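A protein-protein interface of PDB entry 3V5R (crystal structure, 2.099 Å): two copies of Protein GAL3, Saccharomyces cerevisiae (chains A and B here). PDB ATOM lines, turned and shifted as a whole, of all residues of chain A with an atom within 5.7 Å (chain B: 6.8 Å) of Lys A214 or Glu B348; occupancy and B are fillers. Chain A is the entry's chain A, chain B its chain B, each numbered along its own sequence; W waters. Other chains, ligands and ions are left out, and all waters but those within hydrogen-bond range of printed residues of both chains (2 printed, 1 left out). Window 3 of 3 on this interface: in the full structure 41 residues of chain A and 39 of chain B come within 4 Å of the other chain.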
ATOM      1  N   GLU A 210      36.255  27.624   9.861  1.00  0.00           N
ATOM      2  CA  GLU A 210      34.842  27.858  10.122  1.00  0.00           C
ATOM      3  C   GLU A 210      34.059  27.681   8.843  1.00  0.00           C
ATOM      4  O   GLU A 210      34.631  27.749   7.750  1.00  0.00           O
ATOM      5  CB  GLU A 210      34.631  29.289  10.615  1.00  0.00           C
ATOM      6  CG  GLU A 210      35.351  29.625  11.892  1.00  0.00           C
ATOM      7  CD  GLU A 210      35.191  31.104  12.229  1.00  0.00           C
ATOM      8  OE1 GLU A 210      36.065  31.882  11.832  1.00  0.00           O
ATOM      9  OE2 GLU A 210      34.180  31.484  12.854  1.00  0.00           O
ATOM     10  N   PHE A 211      32.750  27.490   8.984  1.00  0.00           N
ATOM     11  CA  PHE A 211      31.863  27.273   7.839  1.00  0.00           C
ATOM     12  C   PHE A 211      30.705  28.279   7.780  1.00  0.00           C
ATOM     13  O   PHE A 211      30.048  28.404   6.742  1.00  0.00           O
ATOM     14  CB  PHE A 211      31.319  25.842   7.865  1.00  0.00           C
ATOM     15  CG  PHE A 211      32.388  24.799   7.956  1.00  0.00           C
ATOM     16  CD1 PHE A 211      33.118  24.442   6.844  1.00  0.00           C
ATOM     17  CD2 PHE A 211      32.658  24.166   9.157  1.00  0.00           C
ATOM     18  CE1 PHE A 211      34.106  23.476   6.923  1.00  0.00           C
ATOM     19  CE2 PHE A 211      33.638  23.191   9.245  1.00  0.00           C
ATOM     20  CZ  PHE A 211      34.373  22.856   8.130  1.00  0.00           C
ATOM     21  N   ARG A 212      30.462  29.001   8.879  1.00  0.00           N
ATOM     22  CA  ARG A 212      29.351  29.971   8.944  1.00  0.00           C
ATOM     23  C   ARG A 212      29.830  31.385   9.275  1.00  0.00           C
ATOM     24  O   ARG A 212      30.562  31.575  10.238  1.00  0.00           O
ATOM     25  CB  ARG A 212      28.317  29.544   9.991  1.00  0.00           C
ATOM     26  CG  ARG A 212      27.808  28.119   9.810  1.00  0.00           C
ATOM     27  CD  ARG A 212      26.631  28.046   8.843  1.00  0.00           C
ATOM     28  NE  ARG A 212      25.541  28.919   9.248  1.00  0.00           N
ATOM     29  CZ  ARG A 212      24.467  28.531   9.935  1.00  0.00           C
ATOM     30  NH1 ARG A 212      24.304  27.255  10.299  1.00  0.00           N
ATOM     31  NH2 ARG A 212      23.542  29.426  10.252  1.00  0.00           N
ATOM     32  N   PRO A 213      29.417  32.389   8.486  1.00  0.00           N
ATOM     33  CA  PRO A 213      28.528  32.303   7.326  1.00  0.00           C
ATOM     34  C   PRO A 213      29.247  31.822   6.089  1.00  0.00           C
ATOM     35  O   PRO A 213      28.583  31.591   5.085  1.00  0.00           O
ATOM     36  CB  PRO A 213      28.104  33.759   7.115  1.00  0.00           C
ATOM     37  CG  PRO A 213      29.306  34.540   7.553  1.00  0.00           C
ATOM     38  CD  PRO A 213      29.827  33.783   8.755  1.00  0.00           C
ATOM     39  N   LYS A 214      30.568  31.654   6.164  1.00  0.00           N
ATOM     40  CA  LYS A 214      31.360  31.260   4.995  1.00  0.00           C
ATOM     41  C   LYS A 214      32.511  30.339   5.393  1.00  0.00           C
ATOM     42  O   LYS A 214      33.009  30.420   6.519  1.00  0.00           O
ATOM     43  CB  LYS A 214      31.977  32.502   4.328  1.00  0.00           C
ATOM     44  CG  LYS A 214      31.011  33.367   3.556  1.00  0.00           C
ATOM     45  CD  LYS A 214      30.802  32.844   2.140  1.00  0.00           C
ATOM     46  CE  LYS A 214      30.048  33.858   1.281  1.00  0.00           C
ATOM     47  NZ  LYS A 214      29.615  33.281  -0.022  1.00  0.00           N
ATOM     48  N   LEU A 215      32.929  29.478   4.473  1.00  0.00           N
ATOM     49  CA  LEU A 215      34.157  28.715   4.646  1.00  0.00           C
ATOM     50  C   LEU A 215      35.285  29.728   4.867  1.00  0.00           C
ATOM     51  O   LEU A 215      35.475  30.625   4.050  1.00  0.00           O
ATOM     52  CB  LEU A 215      34.462  27.919   3.383  1.00  0.00           C
ATOM     53  CG  LEU A 215      35.829  27.210   3.404  1.00  0.00           C
ATOM     54  CD1 LEU A 215      35.875  26.197   4.561  1.00  0.00           C
ATOM     55  CD2 LEU A 215      36.126  26.526   2.054  1.00  0.00           C
ATOM     56  N   LYS A 216      36.031  29.584   5.955  1.00  0.00           N
ATOM     57  CA  LYS A 216      37.033  30.582   6.323  1.00  0.00           C
ATOM     58  C   LYS A 216      38.095  29.926   7.199  1.00  0.00           C
ATOM     59  O   LYS A 216      37.783  29.018   7.971  1.00  0.00           O
ATOM     60  CB  LYS A 216      36.345  31.708   7.110  1.00  0.00           C
ATOM     61  CG  LYS A 216      37.267  32.895   7.453  1.00  0.00           C
ATOM     62  CD  LYS A 216      36.526  33.883   8.354  1.00  0.00           C
ATOM     63  CE  LYS A 216      37.459  34.969   8.899  1.00  0.00           C
ATOM     64  NZ  LYS A 216      38.136  35.787   7.831  1.00  0.00           N
ATOM     65  N   LYS A 277      20.708  31.096   5.312  1.00  0.00           N
ATOM     66  CA  LYS A 277      20.772  32.258   4.416  1.00  0.00           C
ATOM     67  C   LYS A 277      22.161  32.387   3.801  1.00  0.00           C
ATOM     68  O   LYS A 277      22.378  33.165   2.854  1.00  0.00           O
ATOM     69  CB  LYS A 277      20.466  33.544   5.199  1.00  0.00           C
ATOM     70  CG  LYS A 277      19.189  33.497   6.042  1.00  0.00           C
ATOM     71  CD  LYS A 277      17.960  33.216   5.191  1.00  0.00           C
ATOM     72  CE  LYS A 277      16.677  33.512   5.978  1.00  0.00           C
ATOM     73  NZ  LYS A 277      16.671  32.808   7.304  1.00  0.00           N
ATOM     74  N   ASP A 278      23.110  31.656   4.382  1.00  0.00           N
ATOM     75  CA  ASP A 278      24.524  31.735   3.993  1.00  0.00           C
ATOM     76  C   ASP A 278      25.033  30.331   3.621  1.00  0.00           C
ATOM     77  O   ASP A 278      24.264  29.491   3.150  1.00  0.00           O
ATOM     78  CB  ASP A 278      25.355  32.308   5.158  1.00  0.00           C
ATOM     79  CG  ASP A 278      24.670  33.496   5.844  1.00  0.00           C
ATOM     80  OD1 ASP A 278      24.523  34.533   5.168  1.00  0.00           O
ATOM     81  OD2 ASP A 278      24.275  33.399   7.043  1.00  0.00           O
ATOM     82  N   ASN A 279      26.325  30.083   3.835  1.00  0.00           N
ATOM     83  CA  ASN A 279      26.887  28.749   3.655  1.00  0.00           C
ATOM     84  C   ASN A 279      26.406  27.794   4.755  1.00  0.00           C
ATOM     85  O   ASN A 279      26.028  28.241   5.843  1.00  0.00           O
ATOM     86  CB  ASN A 279      28.406  28.817   3.663  1.00  0.00           C
ATOM     87  CG  ASN A 279      29.054  27.485   3.328  1.00  0.00           C
ATOM     88  OD1 ASN A 279      28.744  26.878   2.304  1.00  0.00           O
ATOM     89  ND2 ASN A 279      29.956  27.024   4.194  1.00  0.00           N
ATOM     90  N   SER B 340      23.003  25.705 -10.936  1.00  0.00           N
ATOM     91  CA  SER B 340      22.636  26.852 -10.106  1.00  0.00           C
ATOM     92  C   SER B 340      21.804  27.854 -10.898  1.00  0.00           C
ATOM     93  O   SER B 340      20.817  28.400 -10.403  1.00  0.00           O
ATOM     94  CB  SER B 340      23.875  27.534  -9.542  1.00  0.00           C
ATOM     95  OG  SER B 340      24.658  26.608  -8.821  1.00  0.00           O
ATOM     96  N   CYS B 345      19.643  30.166  -8.417  1.00  0.00           N
ATOM     97  CA  CYS B 345      20.297  30.410  -7.131  1.00  0.00           C
ATOM     98  C   CYS B 345      21.794  30.507  -7.327  1.00  0.00           C
ATOM     99  O   CYS B 345      22.301  30.244  -8.422  1.00  0.00           O
ATOM    100  CB  CYS B 345      19.964  29.285  -6.146  1.00  0.00           C
ATOM    101  SG  CYS B 345      20.702  27.697  -6.589  1.00  0.00           S
ATOM    102  N   SER B 346      22.509  30.882  -6.273  1.00  0.00           N
ATOM    103  CA  SER B 346      23.958  30.975  -6.362  1.00  0.00           C
ATOM    104  C   SER B 346      24.572  29.593  -6.247  1.00  0.00           C
ATOM    105  O   SER B 346      23.919  28.638  -5.825  1.00  0.00           O
ATOM    106  CB  SER B 346      24.508  31.846  -5.240  1.00  0.00           C
ATOM    107  OG  SER B 346      24.229  31.242  -3.986  1.00  0.00           O
ATOM    108  N   ARG B 347      25.840  29.501  -6.611  1.00  0.00           N
ATOM    109  CA  ARG B 347      26.582  28.269  -6.459  1.00  0.00           C
ATOM    110  C   ARG B 347      26.634  27.830  -5.000  1.00  0.00           C
ATOM    111  O   ARG B 347      26.509  26.648  -4.707  1.00  0.00           O
ATOM    112  CB  ARG B 347      28.002  28.429  -6.991  1.00  0.00           C
ATOM    113  CG  ARG B 347      28.746  27.111  -7.032  1.00  0.00           C
ATOM    114  CD  ARG B 347      30.173  27.245  -7.517  1.00  0.00           C
ATOM    115  NE  ARG B 347      30.638  25.987  -8.094  1.00  0.00           N
ATOM    116  CZ  ARG B 347      30.798  25.783  -9.399  1.00  0.00           C
ATOM    117  NH1 ARG B 347      30.550  26.754 -10.266  1.00  0.00           N
ATOM    118  NH2 ARG B 347      31.219  24.611  -9.840  1.00  0.00           N
ATOM    119  N   GLU B 348      26.813  28.787  -4.093  1.00  0.00           N
ATOM    120  CA  GLU B 348      26.886  28.495  -2.665  1.00  0.00           C
ATOM    121  C   GLU B 348      25.589  27.876  -2.167  1.00  0.00           C
ATOM    122  O   GLU B 348      25.611  26.915  -1.406  1.00  0.00           O
ATOM    123  CB  GLU B 348      27.193  29.762  -1.858  1.00  0.00           C
ATOM    124  CG  GLU B 348      26.829  29.651  -0.374  1.00  0.00           C
ATOM    125  CD  GLU B 348      27.244  30.879   0.433  1.00  0.00           C
ATOM    126  OE1 GLU B 348      26.374  31.740   0.699  1.00  0.00           O
ATOM    127  OE2 GLU B 348      28.437  30.981   0.803  1.00  0.00           O
ATOM    128  N   GLU B 349      24.464  28.422  -2.609  1.00  0.00           N
ATOM    129  CA  GLU B 349      23.154  27.887  -2.241  1.00  0.00           C
ATOM    130  C   GLU B 349      22.878  26.550  -2.911  1.00  0.00           C
ATOM    131  O   GLU B 349      22.279  25.650  -2.306  1.00  0.00           O
ATOM    132  CB  GLU B 349      22.051  28.892  -2.565  1.00  0.00           C
ATOM    133  CG  GLU B 349      22.206  30.196  -1.790  1.00  0.00           C
ATOM    134  CD  GLU B 349      21.450  31.367  -2.411  1.00  0.00           C
ATOM    135  OE1 GLU B 349      21.272  31.382  -3.651  1.00  0.00           O
ATOM    136  OE2 GLU B 349      21.045  32.277  -1.653  1.00  0.00           O
ATOM    137  N   PHE B 350      23.309  26.405  -4.159  1.00  0.00           N
ATOM    138  CA  PHE B 350      23.142  25.121  -4.831  1.00  0.00           C
ATOM    139  C   PHE B 350      23.929  24.037  -4.097  1.00  0.00           C
ATOM    140  O   PHE B 350      23.414  22.946  -3.837  1.00  0.00           O
ATOM    141  CB  PHE B 350      23.571  25.174  -6.294  1.00  0.00           C
ATOM    142  CG  PHE B 350      23.391  23.859  -7.009  1.00  0.00           C
ATOM    143  CD1 PHE B 350      22.170  23.529  -7.571  1.00  0.00           C
ATOM    144  CD2 PHE B 350      24.430  22.934  -7.080  1.00  0.00           C
ATOM    145  CE1 PHE B 350      21.988  22.314  -8.210  1.00  0.00           C
ATOM    146  CE2 PHE B 350      24.251  21.710  -7.720  1.00  0.00           C
ATOM    147  CZ  PHE B 350      23.030  21.400  -8.279  1.00  0.00           C
ATOM    148  N   THR B 351      25.184  24.348  -3.795  1.00  0.00           N
ATOM    149  CA  THR B 351      26.089  23.418  -3.124  1.00  0.00           C
ATOM    150  C   THR B 351      25.550  23.007  -1.752  1.00  0.00           C
ATOM    151  O   THR B 351      25.501  21.822  -1.412  1.00  0.00           O
ATOM    152  CB  THR B 351      27.487  24.053  -2.990  1.00  0.00           C
ATOM    153  OG1 THR B 351      28.026  24.263  -4.306  1.00  0.00           O
ATOM    154  CG2 THR B 351      28.439  23.153  -2.191  1.00  0.00           C
ATOM    155  N   ARG B 352      25.149  24.006  -0.974  1.00  0.00           N
ATOM    156  CA  ARG B 352      24.553  23.805   0.336  1.00  0.00           C
ATOM    157  C   ARG B 352      23.312  22.916   0.277  1.00  0.00           C
ATOM    158  O   ARG B 352      23.173  21.969   1.045  1.00  0.00           O
ATOM    159  CB  ARG B 352      24.175  25.166   0.897  1.00  0.00           C
ATOM    160  CG  ARG B 352      23.552  25.156   2.259  1.00  0.00           C
ATOM    161  CD  ARG B 352      23.015  26.557   2.576  1.00  0.00           C
ATOM    162  NE  ARG B 352      21.835  26.841   1.771  1.00  0.00           N
ATOM    163  CZ  ARG B 352      21.387  28.062   1.491  1.00  0.00           C
ATOM    164  NH1 ARG B 352      22.029  29.135   1.932  1.00  0.00           N
ATOM    165  NH2 ARG B 352      20.298  28.204   0.751  1.00  0.00           N
ATOM    166  N   ASP B 353      22.412  23.223  -0.650  1.00  0.00           N
ATOM    167  CA  ASP B 353      21.138  22.524  -0.734  1.00  0.00           C
ATOM    168  C   ASP B 353      21.176  21.163  -1.413  1.00  0.00           C
ATOM    169  O   ASP B 353      20.312  20.324  -1.150  1.00  0.00           O
ATOM    170  CB  ASP B 353      20.090  23.396  -1.416  1.00  0.00           C
ATOM    171  CG  ASP B 353      19.802  24.653  -0.641  1.00  0.00           C
ATOM    172  OD1 ASP B 353      20.111  24.680   0.572  1.00  0.00           O
ATOM    173  OD2 ASP B 353      19.292  25.617  -1.248  1.00  0.00           O
HETATM  174  O   HOH W   1      27.940  26.162  -0.034  1.00  0.00           O
HETATM  175  O   HOH W   2      27.534  33.304   2.943  1.00  0.00           O
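No position is printed for both chains.
Of the 5 pairs that touch across the chains among the printed residues, none has its exchanged pair printed and touching as well.
Printed residues of chain B that touch a printed residue of chain A: Glu B348 and Arg B352.
Of the 10 printed residues of chain A, 4 touch a printed residue of chain B.
Printed residues of chain A that touch a printed residue of chain B: Lys A214, Lys A277, Asp A278 and Asn A279.
Among the printed residues, 5 pairs touch across the chains.
Among the printed residues, Asp or Glu carboxylates within 4 Å of a Lys or Arg side-chain nitrogen of the other chain: Lys A214 with Glu B348 (2.7 Å).
The side-chain amino group of Lys A214 lies within salt-bridge range of the side-chain carboxylate of Glu B348 (2.7 Å).
O of Asp A278 lies within hydrogen-bond range of NH1 of Arg B352, at 2.6 Å.
Of chain B, only Glu B348 (2.7 Å) comes within 4 Å of Lys A214.
Of the printed residues of chain B, Lys A277 touches Arg B352 (3.8 Å).
Printed residues of chain B within 4 Å of Asp A278: Glu B348 (3.5 Å) and Arg B352 (2.6 Å).
Printed residues of chain B within 4 Å of Asn A279: Glu B348.
Of chain A, only Lys A214, Asp A278 and Asn A279 come within 4 Å of Glu B348.
Printed residues of chain A within 4 Å of Arg B352: Lys A277 and Asp A278.
The nearest residue of chain A that does not touch Glu B348 is Pro A213 (4.3 Å).
The nearest printed residue of chain A that does not touch Arg B352 is Asn A279 (4.2 Å).
Water W1 bridges the side-chain amide oxygen (OD1) of Asn A279 and the backbone carbonyl oxygen (O) of Glu B348.
Water W2 lies within hydrogen-bond range of O of Pro A213 and OE1 of Glu B348.
The backbone carbonyl oxygen (O) of Phe A211 lies within hydrogen-bond range of the side-chain amide nitrogen (ND2) of Asn A279, at 2.9 Å.
The backbone carbonyl oxygen (O) of Pro A213 is in hydrogen-bond range of the backbone NH (N) of Asn A279 (3.0 Å).
NE of Arg B352 lies within salt-bridge range of OD1 of Asp B353, at 3.0 Å.
Arg B352 touches Lys A277.
C of Asp A278 touches OE1 of Glu B348 (3.5 Å).
N of Asn A279 touches OE1 of Glu B348 (3.5 Å).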
